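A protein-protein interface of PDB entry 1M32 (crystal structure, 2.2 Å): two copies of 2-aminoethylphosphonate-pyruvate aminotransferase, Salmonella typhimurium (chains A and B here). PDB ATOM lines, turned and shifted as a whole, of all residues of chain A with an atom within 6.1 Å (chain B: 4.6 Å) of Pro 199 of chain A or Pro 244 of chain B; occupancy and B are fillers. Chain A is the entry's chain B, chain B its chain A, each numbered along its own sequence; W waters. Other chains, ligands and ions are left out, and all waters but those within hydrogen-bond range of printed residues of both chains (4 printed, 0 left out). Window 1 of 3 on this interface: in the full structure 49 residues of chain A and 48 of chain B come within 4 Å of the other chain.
Among the printed residues, merely in contact across the chains: Pro 12 of chain A with Thr 242 of chain B (3.7 Å), Met 23 of chain A with His 246 of chain B (3.8 Å), Val 198 of chain A with His 246 of chain B (3.2 Å), Pro 199 of chain A with Thr 242 of chain B (3.7 Å), Pro 199 of chain A with Ser 243 of chain B (3.5 Å), Pro 199 of chain A with Pro 244 of chain B (3.9 Å) and Thr 247 of chain A with Thr 247 of chain B (3.7 Å).
Water W1 bridges OG1 of Thr 242 of chain B (2.6 Å) and ND2 of Asn 192 of chain A (3.1 Å). Water W2 lies within hydrogen-bond range of O of Pro 199 of chain A (2.8 Å) and N of His 246 of chain B (3.2 Å). Water W3 bridges O of Gly 200 of chain A (2.9 Å) and O of Gly 200 of chain B (3.0 Å). Water W4 lies within hydrogen-bond range of the backbone carbonyl oxygen (O) of Gly 200 of chain A (3.0 Å), the backbone carbonyl oxygen (O) of Gly 200 of chain B (3.1 Å) and the backbone NH (N) of Gly 63 of chain A (3.5 Å).
Of the printed residues of chain B, Pro 199 of chain A touches Thr 242, Ser 243 and Pro 244. Printed residues of chain B within 4 Å of Met 23 of chain A: His 246 (3.8 Å). Of the printed residues of chain A, Thr 242 of chain B touches Pro 12 (3.7 Å) and Pro 199 (3.7 Å). The nearest printed residue of chain B that does not touch Pro 199 of chain A is His 246 of chain B (4.01 Å). The nearest residue of chain A that does not touch Pro 244 of chain B is Gly 200 of chain A (4.1 Å). The nearest printed residue of chain B that does not touch Val 198 of chain A is Thr 247 of chain B (5.9 Å).
Of the 11 printed residues of chain B, 5 touch a printed residue of chain A. Hydrophobic or aromatic side chains of chain B that line the printed part of chain A: Pro 244 and His 246. Of the 12 printed residues of chain A, 5 touch a printed residue of chain B. Among the printed residues, 7 pairs touch across the chains. Among the printed residues, no Asp or Glu carboxylate lies within 4 Å of a Lys or Arg side-chain nitrogen of the other chain.
Thr 247 of chain B touches its own counterpart, Thr 247 of chain A. Positions printed for both chains: 200, 201, 244 and 247.
The backbone carbonyl oxygen (O) of Thr 242 of chain B is in hydrogen-bond range of the side-chain amide nitrogen (NE2) of Gln 62 of chain B, at 2.8 Å. The backbone carbonyl oxygen (O) of Pro 244 of chain B is in hydrogen-bond range of the side-chain hydroxyl (OG1) of Thr 247 of chain B (2.7 Å). O of Pro 244 of chain A sits at hydrogen-bond distance from OG1 of Thr 247 of chain A.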
ATOM      1  N   PRO A  12     -23.592  25.406   0.261  1.00  0.00           N
ATOM      2  CA  PRO A  12     -22.953  24.130  -0.091  1.00  0.00           C
ATOM      3  C   PRO A  12     -23.289  23.737  -1.522  1.00  0.00           C
ATOM      4  O   PRO A  12     -24.384  24.020  -2.011  1.00  0.00           O
ATOM      5  CB  PRO A  12     -23.537  23.155   0.931  1.00  0.00           C
ATOM      6  CG  PRO A  12     -23.815  24.031   2.110  1.00  0.00           C
ATOM      7  CD  PRO A  12     -24.433  25.242   1.459  1.00  0.00           C
ATOM      8  N   MET A  23     -13.510  12.298   4.137  1.00  0.00           N
ATOM      9  CA  MET A  23     -14.115  12.515   5.457  1.00  0.00           C
ATOM     10  C   MET A  23     -14.239  11.205   6.248  1.00  0.00           C
ATOM     11  O   MET A  23     -14.425  11.228   7.461  1.00  0.00           O
ATOM     12  CB  MET A  23     -15.531  13.105   5.324  1.00  0.00           C
ATOM     13  CG  MET A  23     -15.677  14.376   4.489  1.00  0.00           C
ATOM     14  SD  MET A  23     -17.424  14.933   4.423  1.00  0.00           S
ATOM     15  CE  MET A  23     -17.489  15.956   5.881  1.00  0.00           C
ATOM     16  N   GLY A  63     -17.739  26.777  12.561  1.00  0.00           N
ATOM     17  CA  GLY A  63     -18.965  27.503  12.260  1.00  0.00           C
ATOM     18  C   GLY A  63     -19.120  27.844  10.789  1.00  0.00           C
ATOM     19  O   GLY A  63     -18.360  27.355   9.950  1.00  0.00           O
ATOM     20  N   ALA A 191     -15.013  27.433   3.287  1.00  0.00           N
ATOM     21  CA  ALA A 191     -14.394  26.154   2.984  1.00  0.00           C
ATOM     22  C   ALA A 191     -15.240  25.393   1.964  1.00  0.00           C
ATOM     23  O   ALA A 191     -14.754  24.457   1.331  1.00  0.00           O
ATOM     24  CB  ALA A 191     -14.259  25.324   4.253  1.00  0.00           C
ATOM     25  N   ASN A 192     -16.496  25.801   1.792  1.00  0.00           N
ATOM     26  CA  ASN A 192     -17.390  25.095   0.873  1.00  0.00           C
ATOM     27  C   ASN A 192     -17.860  25.817  -0.388  1.00  0.00           C
ATOM     28  O   ASN A 192     -18.913  25.476  -0.936  1.00  0.00           O
ATOM     29  CB  ASN A 192     -18.623  24.592   1.630  1.00  0.00           C
ATOM     30  CG  ASN A 192     -19.416  25.717   2.270  1.00  0.00           C
ATOM     31  OD1 ASN A 192     -19.154  26.106   3.408  1.00  0.00           O
ATOM     32  ND2 ASN A 192     -20.387  26.253   1.534  1.00  0.00           N
ATOM     33  N   GLY A 197     -14.770  22.676  -0.884  1.00  0.00           N
ATOM     34  CA  GLY A 197     -14.701  21.772   0.243  1.00  0.00           C
ATOM     35  C   GLY A 197     -16.106  21.575   0.785  1.00  0.00           C
ATOM     36  O   GLY A 197     -17.093  21.818   0.090  1.00  0.00           O
ATOM     37  N   VAL A 198     -16.190  21.151   2.040  1.00  0.00           N
ATOM     38  CA  VAL A 198     -17.457  20.894   2.708  1.00  0.00           C
ATOM     39  C   VAL A 198     -17.644  21.857   3.884  1.00  0.00           C
ATOM     40  O   VAL A 198     -16.675  22.241   4.528  1.00  0.00           O
ATOM     41  CB  VAL A 198     -17.495  19.457   3.238  1.00  0.00           C
ATOM     42  CG1 VAL A 198     -18.265  19.320   4.553  1.00  0.00           C
ATOM     43  CG2 VAL A 198     -18.155  18.483   2.265  1.00  0.00           C
ATOM     44  N   PRO A 199     -18.895  22.270   4.166  1.00  0.00           N
ATOM     45  CA  PRO A 199     -19.136  23.190   5.283  1.00  0.00           C
ATOM     46  C   PRO A 199     -18.758  22.590   6.634  1.00  0.00           C
ATOM     47  O   PRO A 199     -18.751  21.365   6.803  1.00  0.00           O
ATOM     48  CB  PRO A 199     -20.633  23.492   5.170  1.00  0.00           C
ATOM     49  CG  PRO A 199     -21.191  22.263   4.508  1.00  0.00           C
ATOM     50  CD  PRO A 199     -20.150  21.971   3.455  1.00  0.00           C
ATOM     51  N   GLY A 200     -18.440  23.459   7.589  1.00  0.00           N
ATOM     52  CA  GLY A 200     -18.056  23.006   8.915  1.00  0.00           C
ATOM     53  C   GLY A 200     -17.229  24.047   9.646  1.00  0.00           C
ATOM     54  O   GLY A 200     -17.275  24.151  10.873  1.00  0.00           O
ATOM     55  N   PHE A 201     -16.461  24.818   8.886  1.00  0.00           N
ATOM     56  CA  PHE A 201     -15.627  25.867   9.455  1.00  0.00           C
ATOM     57  C   PHE A 201     -15.328  26.876   8.356  1.00  0.00           C
ATOM     58  O   PHE A 201     -15.586  26.619   7.179  1.00  0.00           O
ATOM     59  CB  PHE A 201     -14.305  25.287   9.990  1.00  0.00           C
ATOM     60  CG  PHE A 201     -13.374  24.800   8.908  1.00  0.00           C
ATOM     61  CD1 PHE A 201     -13.593  23.580   8.276  1.00  0.00           C
ATOM     62  CD2 PHE A 201     -12.314  25.596   8.479  1.00  0.00           C
ATOM     63  CE1 PHE A 201     -12.772  23.159   7.226  1.00  0.00           C
ATOM     64  CE2 PHE A 201     -11.485  25.187   7.430  1.00  0.00           C
ATOM     65  CZ  PHE A 201     -11.716  23.967   6.802  1.00  0.00           C
ATOM     66  N   PRO A 244     -14.354  20.419  13.515  1.00  0.00           N
ATOM     67  CA  PRO A 244     -15.046  19.468  12.632  1.00  0.00           C
ATOM     68  C   PRO A 244     -13.997  18.690  11.847  1.00  0.00           C
ATOM     69  O   PRO A 244     -13.874  18.854  10.632  1.00  0.00           O
ATOM     70  CB  PRO A 244     -15.872  20.368  11.706  1.00  0.00           C
ATOM     71  CG  PRO A 244     -15.717  21.770  12.265  1.00  0.00           C
ATOM     72  CD  PRO A 244     -14.392  21.773  12.944  1.00  0.00           C
ATOM     73  N   THR A 247     -14.662  17.364   8.287  1.00  0.00           N
ATOM     74  CA  THR A 247     -14.794  18.397   7.272  1.00  0.00           C
ATOM     75  C   THR A 247     -13.430  19.012   6.971  1.00  0.00           C
ATOM     76  O   THR A 247     -13.210  19.545   5.882  1.00  0.00           O
ATOM     77  CB  THR A 247     -15.754  19.522   7.719  1.00  0.00           C
ATOM     78  OG1 THR A 247     -15.140  20.298   8.757  1.00  0.00           O
ATOM     79  CG2 THR A 247     -17.068  18.926   8.232  1.00  0.00           C
ATOM     80  N   GLN B  62     -24.330  25.807  14.622  1.00  0.00           N
ATOM     81  CA  GLN B  62     -23.040  25.489  14.016  1.00  0.00           C
ATOM     82  C   GLN B  62     -21.907  25.806  14.988  1.00  0.00           C
ATOM     83  O   GLN B  62     -21.990  26.764  15.756  1.00  0.00           O
ATOM     84  CB  GLN B  62     -22.839  26.290  12.721  1.00  0.00           C
ATOM     85  CG  GLN B  62     -23.926  26.097  11.673  1.00  0.00           C
ATOM     86  CD  GLN B  62     -25.056  27.100  11.804  1.00  0.00           C
ATOM     87  OE1 GLN B  62     -25.554  27.356  12.898  1.00  0.00           O
ATOM     88  NE2 GLN B  62     -25.476  27.668  10.677  1.00  0.00           N
ATOM     89  N   GLY B 200     -19.284  19.270  14.344  1.00  0.00           N
ATOM     90  CA  GLY B 200     -19.813  20.132  13.300  1.00  0.00           C
ATOM     91  C   GLY B 200     -20.795  21.147  13.848  1.00  0.00           C
ATOM     92  O   GLY B 200     -20.820  22.307  13.430  1.00  0.00           O
ATOM     93  N   PHE B 201     -21.614  20.702  14.792  1.00  0.00           N
ATOM     94  CA  PHE B 201     -22.601  21.566  15.412  1.00  0.00           C
ATOM     95  C   PHE B 201     -22.940  21.008  16.785  1.00  0.00           C
ATOM     96  O   PHE B 201     -22.569  19.881  17.119  1.00  0.00           O
ATOM     97  CB  PHE B 201     -23.879  21.626  14.560  1.00  0.00           C
ATOM     98  CG  PHE B 201     -24.635  20.319  14.505  1.00  0.00           C
ATOM     99  CD1 PHE B 201     -24.173  19.262  13.724  1.00  0.00           C
ATOM    100  CD2 PHE B 201     -25.779  20.133  15.272  1.00  0.00           C
ATOM    101  CE1 PHE B 201     -24.834  18.031  13.711  1.00  0.00           C
ATOM    102  CE2 PHE B 201     -26.452  18.907  15.271  1.00  0.00           C
ATOM    103  CZ  PHE B 201     -25.978  17.853  14.488  1.00  0.00           C
ATOM    104  N   TRP B 239     -31.849  26.541   8.669  1.00  0.00           N
ATOM    105  CA  TRP B 239     -30.796  27.161   9.471  1.00  0.00           C
ATOM    106  C   TRP B 239     -30.582  28.555   8.868  1.00  0.00           C
ATOM    107  O   TRP B 239     -30.517  28.689   7.646  1.00  0.00           O
ATOM    108  CB  TRP B 239     -29.476  26.390   9.351  1.00  0.00           C
ATOM    109  CG  TRP B 239     -29.476  24.961   9.817  1.00  0.00           C
ATOM    110  CD1 TRP B 239     -30.208  23.925   9.305  1.00  0.00           C
ATOM    111  CD2 TRP B 239     -28.610  24.388  10.806  1.00  0.00           C
ATOM    112  NE1 TRP B 239     -29.840  22.742   9.906  1.00  0.00           N
ATOM    113  CE2 TRP B 239     -28.862  22.999  10.832  1.00  0.00           C
ATOM    114  CE3 TRP B 239     -27.638  24.915  11.669  1.00  0.00           C
ATOM    115  CZ2 TRP B 239     -28.177  22.128  11.688  1.00  0.00           C
ATOM    116  CZ3 TRP B 239     -26.956  24.049  12.519  1.00  0.00           C
ATOM    117  CH2 TRP B 239     -27.231  22.671  12.521  1.00  0.00           C
ATOM    118  N   THR B 242     -25.325  28.898   6.591  1.00  0.00           N
ATOM    119  CA  THR B 242     -24.883  27.591   6.116  1.00  0.00           C
ATOM    120  C   THR B 242     -24.685  26.627   7.278  1.00  0.00           C
ATOM    121  O   THR B 242     -24.095  26.981   8.303  1.00  0.00           O
ATOM    122  CB  THR B 242     -23.550  27.692   5.356  1.00  0.00           C
ATOM    123  OG1 THR B 242     -23.719  28.527   4.206  1.00  0.00           O
ATOM    124  CG2 THR B 242     -23.076  26.313   4.920  1.00  0.00           C
ATOM    125  N   SER B 243     -25.183  25.407   7.111  1.00  0.00           N
ATOM    126  CA  SER B 243     -25.047  24.380   8.134  1.00  0.00           C
ATOM    127  C   SER B 243     -24.124  23.286   7.613  1.00  0.00           C
ATOM    128  O   SER B 243     -24.007  23.092   6.400  1.00  0.00           O
ATOM    129  CB  SER B 243     -26.413  23.778   8.466  1.00  0.00           C
ATOM    130  OG  SER B 243     -26.976  23.134   7.335  1.00  0.00           O
ATOM    131  N   PRO B 244     -23.448  22.566   8.523  1.00  0.00           N
ATOM    132  CA  PRO B 244     -22.538  21.487   8.126  1.00  0.00           C
ATOM    133  C   PRO B 244     -23.379  20.269   7.759  1.00  0.00           C
ATOM    134  O   PRO B 244     -23.412  19.276   8.487  1.00  0.00           O
ATOM    135  CB  PRO B 244     -21.696  21.276   9.384  1.00  0.00           C
ATOM    136  CG  PRO B 244     -22.683  21.538  10.485  1.00  0.00           C
ATOM    137  CD  PRO B 244     -23.436  22.761   9.988  1.00  0.00           C
ATOM    138  N   THR B 245     -24.059  20.364   6.620  1.00  0.00           N
ATOM    139  CA  THR B 245     -24.956  19.316   6.146  1.00  0.00           C
ATOM    140  C   THR B 245     -24.458  17.880   6.262  1.00  0.00           C
ATOM    141  O   THR B 245     -25.199  17.007   6.697  1.00  0.00           O
ATOM    142  CB  THR B 245     -25.360  19.556   4.686  1.00  0.00           C
ATOM    143  OG1 THR B 245     -24.203  19.461   3.851  1.00  0.00           O
ATOM    144  CG2 THR B 245     -25.993  20.931   4.527  1.00  0.00           C
ATOM    145  N   HIS B 246     -23.216  17.631   5.869  1.00  0.00           N
ATOM    146  CA  HIS B 246     -22.672  16.278   5.929  1.00  0.00           C
ATOM    147  C   HIS B 246     -22.619  15.746   7.355  1.00  0.00           C
ATOM    148  O   HIS B 246     -22.885  14.567   7.584  1.00  0.00           O
ATOM    149  CB  HIS B 246     -21.277  16.251   5.301  1.00  0.00           C
ATOM    150  CG  HIS B 246     -21.241  16.820   3.918  1.00  0.00           C
ATOM    151  ND1 HIS B 246     -21.316  16.037   2.786  1.00  0.00           N
ATOM    152  CD2 HIS B 246     -21.214  18.102   3.484  1.00  0.00           C
ATOM    153  CE1 HIS B 246     -21.338  16.811   1.717  1.00  0.00           C
ATOM    154  NE2 HIS B 246     -21.278  18.069   2.113  1.00  0.00           N
ATOM    155  N   THR B 247     -22.276  16.610   8.308  1.00  0.00           N
ATOM    156  CA  THR B 247     -22.203  16.188   9.700  1.00  0.00           C
ATOM    157  C   THR B 247     -23.607  16.012  10.260  1.00  0.00           C
ATOM    158  O   THR B 247     -23.817  15.219  11.178  1.00  0.00           O
ATOM    159  CB  THR B 247     -21.429  17.207  10.573  1.00  0.00           C
ATOM    160  OG1 THR B 247     -22.223  18.380  10.778  1.00  0.00           O
ATOM    161  CG2 THR B 247     -20.119  17.587   9.895  1.00  0.00           C
ATOM    162  N   VAL B 248     -24.562  16.756   9.706  1.00  0.00           N
ATOM    163  CA  VAL B 248     -25.955  16.666  10.131  1.00  0.00           C
ATOM    164  C   VAL B 248     -26.534  15.329   9.658  1.00  0.00           C
ATOM    165  O   VAL B 248     -27.319  14.698  10.360  1.00  0.00           O
ATOM    166  CB  VAL B 248     -26.796  17.834   9.554  1.00  0.00           C
ATOM    167  CG1 VAL B 248     -28.268  17.631   9.874  1.00  0.00           C
ATOM    168  CG2 VAL B 248     -26.316  19.160  10.146  1.00  0.00           C
HETATM  169  O   HOH W   1     -21.969  28.796   2.246  1.00  0.00           O
HETATM  170  O   HOH W   2     -20.548  19.265   6.443  1.00  0.00           O
HETATM  171  O   HOH W   3     -17.984  23.322  13.526  1.00  0.00           O
HETATM  172  O   HOH W   4     -20.221  24.631  11.408  1.00  0.00           O
